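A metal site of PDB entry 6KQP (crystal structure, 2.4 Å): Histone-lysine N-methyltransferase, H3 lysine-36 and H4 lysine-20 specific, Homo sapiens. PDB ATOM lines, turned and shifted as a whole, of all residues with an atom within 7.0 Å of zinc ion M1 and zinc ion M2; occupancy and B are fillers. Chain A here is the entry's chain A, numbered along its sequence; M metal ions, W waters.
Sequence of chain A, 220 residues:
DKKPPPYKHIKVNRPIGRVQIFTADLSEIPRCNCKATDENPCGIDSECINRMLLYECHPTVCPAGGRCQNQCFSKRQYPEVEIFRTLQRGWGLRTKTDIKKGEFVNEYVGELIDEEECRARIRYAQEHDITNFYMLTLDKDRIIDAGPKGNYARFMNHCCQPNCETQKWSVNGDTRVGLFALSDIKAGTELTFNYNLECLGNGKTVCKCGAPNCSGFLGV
The side-chain hydroxyl (OG) of Ser 46 sits at hydrogen-bond distance from the backbone NH (N) of Cys 48. The backbone NH (N) of Arg 51 sits close to the side-chain sulfur (SG) of Cys 48, at 3.5 Å. The backbone carbonyl oxygen (O) of Cys 42 sits at hydrogen-bond distance from the guanidinium group (NE) of Arg 51 (2.8 Å). The backbone NH (N) of Asn 50 sits close to the side-chain sulfur (SG) of Cys 48, at 3.7 Å. The backbone NH of Cys 32 lies within hydrogen-bond range of the side-chain amide oxygen of Asn 50 (2.9 Å). SG of Cys 68 sits close to NE2 of Gln 71 (3.3 Å). The backbone NH of Ala 64 lies close to the side-chain sulfur of Cys 62 (3.7 Å). The side-chain sulfur (SG) of Cys 68 sits close to the backbone NH (N) of Asn 70, at 3.4 Å.
Of the 27 residues printed, 4 come within 4 Å of zinc ion M1. The nearest printed residue that does not touch zinc ion M1 is Asn 70 (4.2 Å).
Of the 27 residues printed, 5 come within 4 Å of zinc ion M2. Along chain A the residues within 4 Å of zinc ion M2 span positions 32 to 57. The nearest printed residue that does not touch zinc ion M2 is Cys 62 (4.4 Å).
Zinc ion M1 is bound by the side-chain sulfur (SG) of Cys 42 (2.1 Å), the side-chain sulfur (SG) of Cys 68 (2.2 Å), the side-chain sulfur (SG) of Cys 62 (2.4 Å) and the side-chain sulfur (SG) of Cys 57 (2.4 Å).
Zinc ion M2 is bound by SG of Cys 32 (2.1 Å), SG of Cys 48 (2.3 Å), SG of Cys 42 (2.3 Å) and SG of Cys 34 (2.4 Å).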
ATOM      1  N   ARG A  31      18.824  -8.992  -2.890  1.00  0.00           N
ATOM      2  CA  ARG A  31      17.961  -7.818  -3.132  1.00  0.00           C
ATOM      3  C   ARG A  31      18.333  -6.709  -2.148  1.00  0.00           C
ATOM      4  O   ARG A  31      18.407  -6.982  -0.967  1.00  0.00           O
ATOM      5  CB  ARG A  31      16.507  -8.218  -2.949  1.00  0.00           C
ATOM      6  CG  ARG A  31      15.935  -8.905  -4.179  1.00  0.00           C
ATOM      7  CD  ARG A  31      14.702  -9.682  -3.770  1.00  0.00           C
ATOM      8  NE  ARG A  31      13.999 -10.217  -4.921  1.00  0.00           N
ATOM      9  CZ  ARG A  31      14.214 -11.404  -5.433  1.00  0.00           C
ATOM     10  NH1 ARG A  31      15.130 -12.195  -4.894  1.00  0.00           N
ATOM     11  NH2 ARG A  31      13.513 -11.820  -6.468  1.00  0.00           N
ATOM     12  N   CYS A  32      18.550  -5.507  -2.643  1.00  0.00           N
ATOM     13  CA  CYS A  32      18.920  -4.372  -1.776  1.00  0.00           C
ATOM     14  C   CYS A  32      17.686  -3.691  -1.170  1.00  0.00           C
ATOM     15  O   CYS A  32      16.573  -4.050  -1.515  1.00  0.00           O
ATOM     16  CB  CYS A  32      19.867  -3.420  -2.464  1.00  0.00           C
ATOM     17  SG  CYS A  32      19.100  -2.075  -3.374  1.00  0.00           S
ATOM     18  N   ASN A  33      17.924  -2.797  -0.223  1.00  0.00           N
ATOM     19  CA  ASN A  33      16.810  -2.064   0.420  1.00  0.00           C
ATOM     20  C   ASN A  33      16.913  -0.563   0.145  1.00  0.00           C
ATOM     21  O   ASN A  33      16.296   0.181   0.878  1.00  0.00           O
ATOM     22  CB  ASN A  33      16.690  -2.385   1.909  1.00  0.00           C
ATOM     23  CG  ASN A  33      15.322  -2.025   2.451  1.00  0.00           C
ATOM     24  OD1 ASN A  33      14.321  -2.292   1.819  1.00  0.00           O
ATOM     25  ND2 ASN A  33      15.288  -1.412   3.619  1.00  0.00           N
ATOM     26  N   CYS A  34      17.491  -0.146  -0.985  1.00  0.00           N
ATOM     27  CA  CYS A  34      17.484   1.285  -1.368  1.00  0.00           C
ATOM     28  C   CYS A  34      16.060   1.686  -1.790  1.00  0.00           C
ATOM     29  O   CYS A  34      15.209   0.806  -2.100  1.00  0.00           O
ATOM     30  CB  CYS A  34      18.503   1.547  -2.464  1.00  0.00           C
ATOM     31  SG  CYS A  34      20.183   0.975  -2.059  1.00  0.00           S
ATOM     32  N   LYS A  35      15.790   2.975  -1.815  1.00  0.00           N
ATOM     33  CA  LYS A  35      14.478   3.489  -2.292  1.00  0.00           C
ATOM     34  C   LYS A  35      14.731   4.399  -3.505  1.00  0.00           C
ATOM     35  O   LYS A  35      15.738   5.110  -3.506  1.00  0.00           O
ATOM     36  CB  LYS A  35      13.738   4.192  -1.140  1.00  0.00           C
ATOM     37  CG  LYS A  35      13.465   3.296   0.049  1.00  0.00           C
ATOM     38  CD  LYS A  35      13.252   4.003   1.362  1.00  0.00           C
ATOM     39  CE  LYS A  35      12.957   3.017   2.489  1.00  0.00           C
ATOM     40  NZ  LYS A  35      11.879   3.485   3.386  1.00  0.00           N
ATOM     41  N   ASP A  38      15.899   7.787  -2.668  1.00  0.00           N
ATOM     42  CA  ASP A  38      17.248   8.045  -2.069  1.00  0.00           C
ATOM     43  C   ASP A  38      17.975   9.021  -3.011  1.00  0.00           C
ATOM     44  O   ASP A  38      17.570   9.122  -4.185  1.00  0.00           O
ATOM     45  CB  ASP A  38      18.100   6.789  -1.863  1.00  0.00           C
ATOM     46  CG  ASP A  38      17.513   5.747  -0.910  1.00  0.00           C
ATOM     47  OD1 ASP A  38      16.592   6.105  -0.144  1.00  0.00           O
ATOM     48  OD2 ASP A  38      17.962   4.573  -0.955  1.00  0.00           O
ATOM     49  N   PRO A  41      20.301   6.451  -5.633  1.00  0.00           N
ATOM     50  CA  PRO A  41      19.873   5.089  -5.289  1.00  0.00           C
ATOM     51  C   PRO A  41      20.911   4.063  -5.762  1.00  0.00           C
ATOM     52  O   PRO A  41      21.293   4.136  -6.915  1.00  0.00           O
ATOM     53  CB  PRO A  41      18.532   4.936  -6.035  1.00  0.00           C
ATOM     54  CG  PRO A  41      18.042   6.356  -6.244  1.00  0.00           C
ATOM     55  CD  PRO A  41      19.308   7.177  -6.431  1.00  0.00           C
ATOM     56  N   CYS A  42      21.355   3.184  -4.862  1.00  0.00           N
ATOM     57  CA  CYS A  42      22.360   2.124  -5.131  1.00  0.00           C
ATOM     58  C   CYS A  42      23.701   2.727  -5.583  1.00  0.00           C
ATOM     59  O   CYS A  42      24.542   2.009  -6.090  1.00  0.00           O
ATOM     60  CB  CYS A  42      21.808   1.143  -6.156  1.00  0.00           C
ATOM     61  SG  CYS A  42      20.186   0.449  -5.688  1.00  0.00           S
ATOM     62  N   GLY A  43      23.908   4.027  -5.393  1.00  0.00           N
ATOM     63  CA  GLY A  43      25.118   4.714  -5.866  1.00  0.00           C
ATOM     64  C   GLY A  43      26.300   4.419  -4.972  1.00  0.00           C
ATOM     65  O   GLY A  43      26.115   3.752  -3.937  1.00  0.00           O
ATOM     66  N   SER A  46      26.037   5.099  -1.280  1.00  0.00           N
ATOM     67  CA  SER A  46      24.813   4.558  -0.649  1.00  0.00           C
ATOM     68  C   SER A  46      25.196   3.407   0.291  1.00  0.00           C
ATOM     69  O   SER A  46      26.359   3.011   0.263  1.00  0.00           O
ATOM     70  CB  SER A  46      23.811   4.085  -1.684  1.00  0.00           C
ATOM     71  OG  SER A  46      24.195   2.833  -2.216  1.00  0.00           O
ATOM     72  N   GLU A  47      24.220   2.857   0.997  1.00  0.00           N
ATOM     73  CA  GLU A  47      24.380   1.668   1.882  1.00  0.00           C
ATOM     74  C   GLU A  47      23.826   0.433   1.169  1.00  0.00           C
ATOM     75  O   GLU A  47      23.452  -0.522   1.861  1.00  0.00           O
ATOM     76  CB  GLU A  47      23.653   1.890   3.213  1.00  0.00           C
ATOM     77  CG  GLU A  47      23.895   3.255   3.856  1.00  0.00           C
ATOM     78  CD  GLU A  47      24.759   3.287   5.113  1.00  0.00           C
ATOM     79  OE1 GLU A  47      24.947   4.393   5.674  1.00  0.00           O
ATOM     80  OE2 GLU A  47      25.230   2.204   5.557  1.00  0.00           O
ATOM     81  N   CYS A  48      23.738   0.454  -0.165  1.00  0.00           N
ATOM     82  CA  CYS A  48      23.218  -0.670  -0.982  1.00  0.00           C
ATOM     83  C   CYS A  48      23.913  -1.978  -0.561  1.00  0.00           C
ATOM     84  O   CYS A  48      25.154  -2.056  -0.641  1.00  0.00           O
ATOM     85  CB  CYS A  48      23.426  -0.403  -2.464  1.00  0.00           C
ATOM     86  SG  CYS A  48      22.708  -1.684  -3.528  1.00  0.00           S
ATOM     87  N   ILE A  49      23.141  -2.955  -0.089  1.00  0.00           N
ATOM     88  CA  ILE A  49      23.719  -4.230   0.394  1.00  0.00           C
ATOM     89  C   ILE A  49      24.370  -4.922  -0.802  1.00  0.00           C
ATOM     90  O   ILE A  49      25.509  -5.407  -0.647  1.00  0.00           O
ATOM     91  CB  ILE A  49      22.675  -5.113   1.124  1.00  0.00           C
ATOM     92  CG1 ILE A  49      23.321  -6.391   1.696  1.00  0.00           C
ATOM     93  CG2 ILE A  49      21.486  -5.467   0.260  1.00  0.00           C
ATOM     94  CD1 ILE A  49      24.473  -6.127   2.659  1.00  0.00           C
ATOM     95  N   ASN A  50      23.694  -4.937  -1.973  1.00  0.00           N
ATOM     96  CA  ASN A  50      24.233  -5.530  -3.218  1.00  0.00           C
ATOM     97  C   ASN A  50      25.601  -4.905  -3.492  1.00  0.00           C
ATOM     98  O   ASN A  50      26.589  -5.657  -3.677  1.00  0.00           O
ATOM     99  CB  ASN A  50      23.301  -5.324  -4.392  1.00  0.00           C
ATOM    100  CG  ASN A  50      22.017  -6.121  -4.250  1.00  0.00           C
ATOM    101  OD1 ASN A  50      21.382  -6.062  -3.217  1.00  0.00           O
ATOM    102  ND2 ASN A  50      21.676  -6.928  -5.226  1.00  0.00           N
ATOM    103  N   ARG A  51      25.681  -3.580  -3.468  1.00  0.00           N
ATOM    104  CA  ARG A  51      26.952  -2.870  -3.781  1.00  0.00           C
ATOM    105  C   ARG A  51      28.019  -3.305  -2.772  1.00  0.00           C
ATOM    106  O   ARG A  51      29.163  -3.550  -3.183  1.00  0.00           O
ATOM    107  CB  ARG A  51      26.726  -1.354  -3.790  1.00  0.00           C
ATOM    108  CG  ARG A  51      27.936  -0.597  -4.319  1.00  0.00           C
ATOM    109  CD  ARG A  51      27.715   0.885  -4.376  1.00  0.00           C
ATOM    110  NE  ARG A  51      27.275   1.349  -5.696  1.00  0.00           N
ATOM    111  CZ  ARG A  51      28.052   1.500  -6.753  1.00  0.00           C
ATOM    112  NH1 ARG A  51      29.331   1.160  -6.713  1.00  0.00           N
ATOM    113  NH2 ARG A  51      27.539   1.952  -7.870  1.00  0.00           N
ATOM    114  N   GLU A  56      25.902  -6.703  -8.498  1.00  0.00           N
ATOM    115  CA  GLU A  56      24.996  -5.767  -9.191  1.00  0.00           C
ATOM    116  C   GLU A  56      23.583  -5.953  -8.632  1.00  0.00           C
ATOM    117  O   GLU A  56      23.241  -7.073  -8.188  1.00  0.00           O
ATOM    118  CB  GLU A  56      24.983  -6.012 -10.702  1.00  0.00           C
ATOM    119  CG  GLU A  56      26.141  -5.365 -11.427  1.00  0.00           C
ATOM    120  CD  GLU A  56      25.947  -5.242 -12.930  1.00  0.00           C
ATOM    121  OE1 GLU A  56      24.885  -5.705 -13.446  1.00  0.00           O
ATOM    122  OE2 GLU A  56      26.837  -4.667 -13.591  1.00  0.00           O
ATOM    123  N   CYS A  57      22.804  -4.880  -8.594  1.00  0.00           N
ATOM    124  CA  CYS A  57      21.338  -4.935  -8.408  1.00  0.00           C
ATOM    125  C   CYS A  57      20.860  -5.547  -9.741  1.00  0.00           C
ATOM    126  O   CYS A  57      21.429  -5.198 -10.796  1.00  0.00           O
ATOM    127  CB  CYS A  57      20.759  -3.549  -8.081  1.00  0.00           C
ATOM    128  SG  CYS A  57      20.991  -2.866  -6.395  1.00  0.00           S
ATOM    129  N   HIS A  58      19.940  -6.508  -9.733  1.00  0.00           N
ATOM    130  CA  HIS A  58      19.261  -6.950 -10.978  1.00  0.00           C
ATOM    131  C   HIS A  58      18.110  -5.995 -11.298  1.00  0.00           C
ATOM    132  O   HIS A  58      17.300  -5.670 -10.428  1.00  0.00           O
ATOM    133  CB  HIS A  58      18.784  -8.394 -10.890  1.00  0.00           C
ATOM    134  CG  HIS A  58      18.399  -8.917 -12.228  1.00  0.00           C
ATOM    135  ND1 HIS A  58      17.186  -8.630 -12.799  1.00  0.00           N
ATOM    136  CD2 HIS A  58      19.086  -9.626 -13.147  1.00  0.00           C
ATOM    137  CE1 HIS A  58      17.125  -9.179 -14.000  1.00  0.00           C
ATOM    138  NE2 HIS A  58      18.281  -9.800 -14.228  1.00  0.00           N
ATOM    139  N   CYS A  62      15.278  -4.557  -8.500  1.00  0.00           N
ATOM    140  CA  CYS A  62      15.857  -3.526  -7.594  1.00  0.00           C
ATOM    141  C   CYS A  62      14.746  -2.567  -7.211  1.00  0.00           C
ATOM    142  O   CYS A  62      14.123  -1.950  -8.062  1.00  0.00           O
ATOM    143  CB  CYS A  62      17.038  -2.773  -8.158  1.00  0.00           C
ATOM    144  SG  CYS A  62      17.819  -1.726  -6.902  1.00  0.00           S
ATOM    145  N   PRO A  63      14.464  -2.411  -5.904  1.00  0.00           N
ATOM    146  CA  PRO A  63      13.393  -1.512  -5.470  1.00  0.00           C
ATOM    147  C   PRO A  63      13.600  -0.059  -5.968  1.00  0.00           C
ATOM    148  O   PRO A  63      12.639   0.689  -5.926  1.00  0.00           O
ATOM    149  CB  PRO A  63      13.398  -1.636  -3.933  1.00  0.00           C
ATOM    150  CG  PRO A  63      14.771  -2.183  -3.589  1.00  0.00           C
ATOM    151  CD  PRO A  63      15.163  -3.054  -4.766  1.00  0.00           C
ATOM    152  N   ALA A  64      14.780   0.314  -6.479  1.00  0.00           N
ATOM    153  CA  ALA A  64      15.067   1.684  -6.970  1.00  0.00           C
ATOM    154  C   ALA A  64      14.786   1.830  -8.474  1.00  0.00           C
ATOM    155  O   ALA A  64      15.055   2.932  -9.050  1.00  0.00           O
ATOM    156  CB  ALA A  64      16.492   2.052  -6.691  1.00  0.00           C
ATOM    157  N   GLY A  65      14.323   0.750  -9.114  1.00  0.00           N
ATOM    158  CA  GLY A  65      13.883   0.786 -10.518  1.00  0.00           C
ATOM    159  C   GLY A  65      14.952   1.354 -11.440  1.00  0.00           C
ATOM    160  O   GLY A  65      16.164   0.986 -11.259  1.00  0.00           O
ATOM    161  N   ARG A  67      16.307   4.172 -11.558  1.00  0.00           N
ATOM    162  CA  ARG A  67      17.280   5.099 -10.907  1.00  0.00           C
ATOM    163  C   ARG A  67      18.477   4.320 -10.327  1.00  0.00           C
ATOM    164  O   ARG A  67      19.450   4.978  -9.887  1.00  0.00           O
ATOM    165  CB  ARG A  67      16.583   5.931  -9.846  1.00  0.00           C
ATOM    166  CG  ARG A  67      15.520   6.830 -10.428  1.00  0.00           C
ATOM    167  CD  ARG A  67      14.945   7.724  -9.354  1.00  0.00           C
ATOM    168  NE  ARG A  67      13.834   8.494  -9.880  1.00  0.00           N
ATOM    169  CZ  ARG A  67      13.196   9.446  -9.215  1.00  0.00           C
ATOM    170  NH1 ARG A  67      13.568   9.771  -7.984  1.00  0.00           N
ATOM    171  NH2 ARG A  67      12.192  10.093  -9.782  1.00  0.00           N
ATOM    172  N   CYS A  68      18.410   2.993 -10.310  1.00  0.00           N
ATOM    173  CA  CYS A  68      19.477   2.144  -9.735  1.00  0.00           C
ATOM    174  C   CYS A  68      20.818   2.499 -10.390  1.00  0.00           C
ATOM    175  O   CYS A  68      20.894   2.493 -11.608  1.00  0.00           O
ATOM    176  CB  CYS A  68      19.113   0.669  -9.902  1.00  0.00           C
ATOM    177  SG  CYS A  68      20.438  -0.471  -9.468  1.00  0.00           S
ATOM    178  N   GLN A  69      21.829   2.823  -9.595  1.00  0.00           N
ATOM    179  CA  GLN A  69      23.201   3.138 -10.061  1.00  0.00           C
ATOM    180  C   GLN A  69      24.146   1.941  -9.853  1.00  0.00           C
ATOM    181  O   GLN A  69      25.343   2.155  -9.914  1.00  0.00           O
ATOM    182  CB  GLN A  69      23.689   4.371  -9.311  1.00  0.00           C
ATOM    183  CG  GLN A  69      22.915   5.620  -9.670  1.00  0.00           C
ATOM    184  CD  GLN A  69      23.408   6.802  -8.887  1.00  0.00           C
ATOM    185  OE1 GLN A  69      24.502   6.783  -8.318  1.00  0.00           O
ATOM    186  NE2 GLN A  69      22.577   7.838  -8.810  1.00  0.00           N
ATOM    187  N   ASN A  70      23.628   0.728  -9.690  1.00  0.00           N
ATOM    188  CA  ASN A  70      24.463  -0.466  -9.379  1.00  0.00           C
ATOM    189  C   ASN A  70      24.293  -1.490 -10.495  1.00  0.00           C
ATOM    190  O   ASN A  70      23.931  -2.632 -10.179  1.00  0.00           O
ATOM    191  CB  ASN A  70      24.092  -1.081  -8.027  1.00  0.00           C
ATOM    192  CG  ASN A  70      25.112  -2.097  -7.524  1.00  0.00           C
ATOM    193  OD1 ASN A  70      26.289  -2.016  -7.874  1.00  0.00           O
ATOM    194  ND2 ASN A  70      24.674  -3.008  -6.668  1.00  0.00           N
ATOM    195  N   GLN A  71      24.475  -1.070 -11.747  1.00  0.00           N
ATOM    196  CA  GLN A  71      24.464  -1.981 -12.918  1.00  0.00           C
ATOM    197  C   GLN A  71      25.636  -1.657 -13.839  1.00  0.00           C
ATOM    198  O   GLN A  71      25.478  -1.851 -15.069  1.00  0.00           O
ATOM    199  CB  GLN A  71      23.132  -1.887 -13.636  1.00  0.00           C
ATOM    200  CG  GLN A  71      21.993  -2.528 -12.880  1.00  0.00           C
ATOM    201  CD  GLN A  71      20.668  -2.086 -13.430  1.00  0.00           C
ATOM    202  OE1 GLN A  71      20.427  -2.226 -14.630  1.00  0.00           O
ATOM    203  NE2 GLN A  71      19.821  -1.546 -12.569  1.00  0.00           N
HETATM  204 ZN    ZN M   1      19.996  -0.925  -7.325  1.00  0.00          ZN
HETATM  205 ZN    ZN M   2      20.657  -0.653  -3.695  1.00  0.00          ZN
HETATM  206  O   HOH W   1      18.777  -3.559  -5.649  1.00  0.00           O
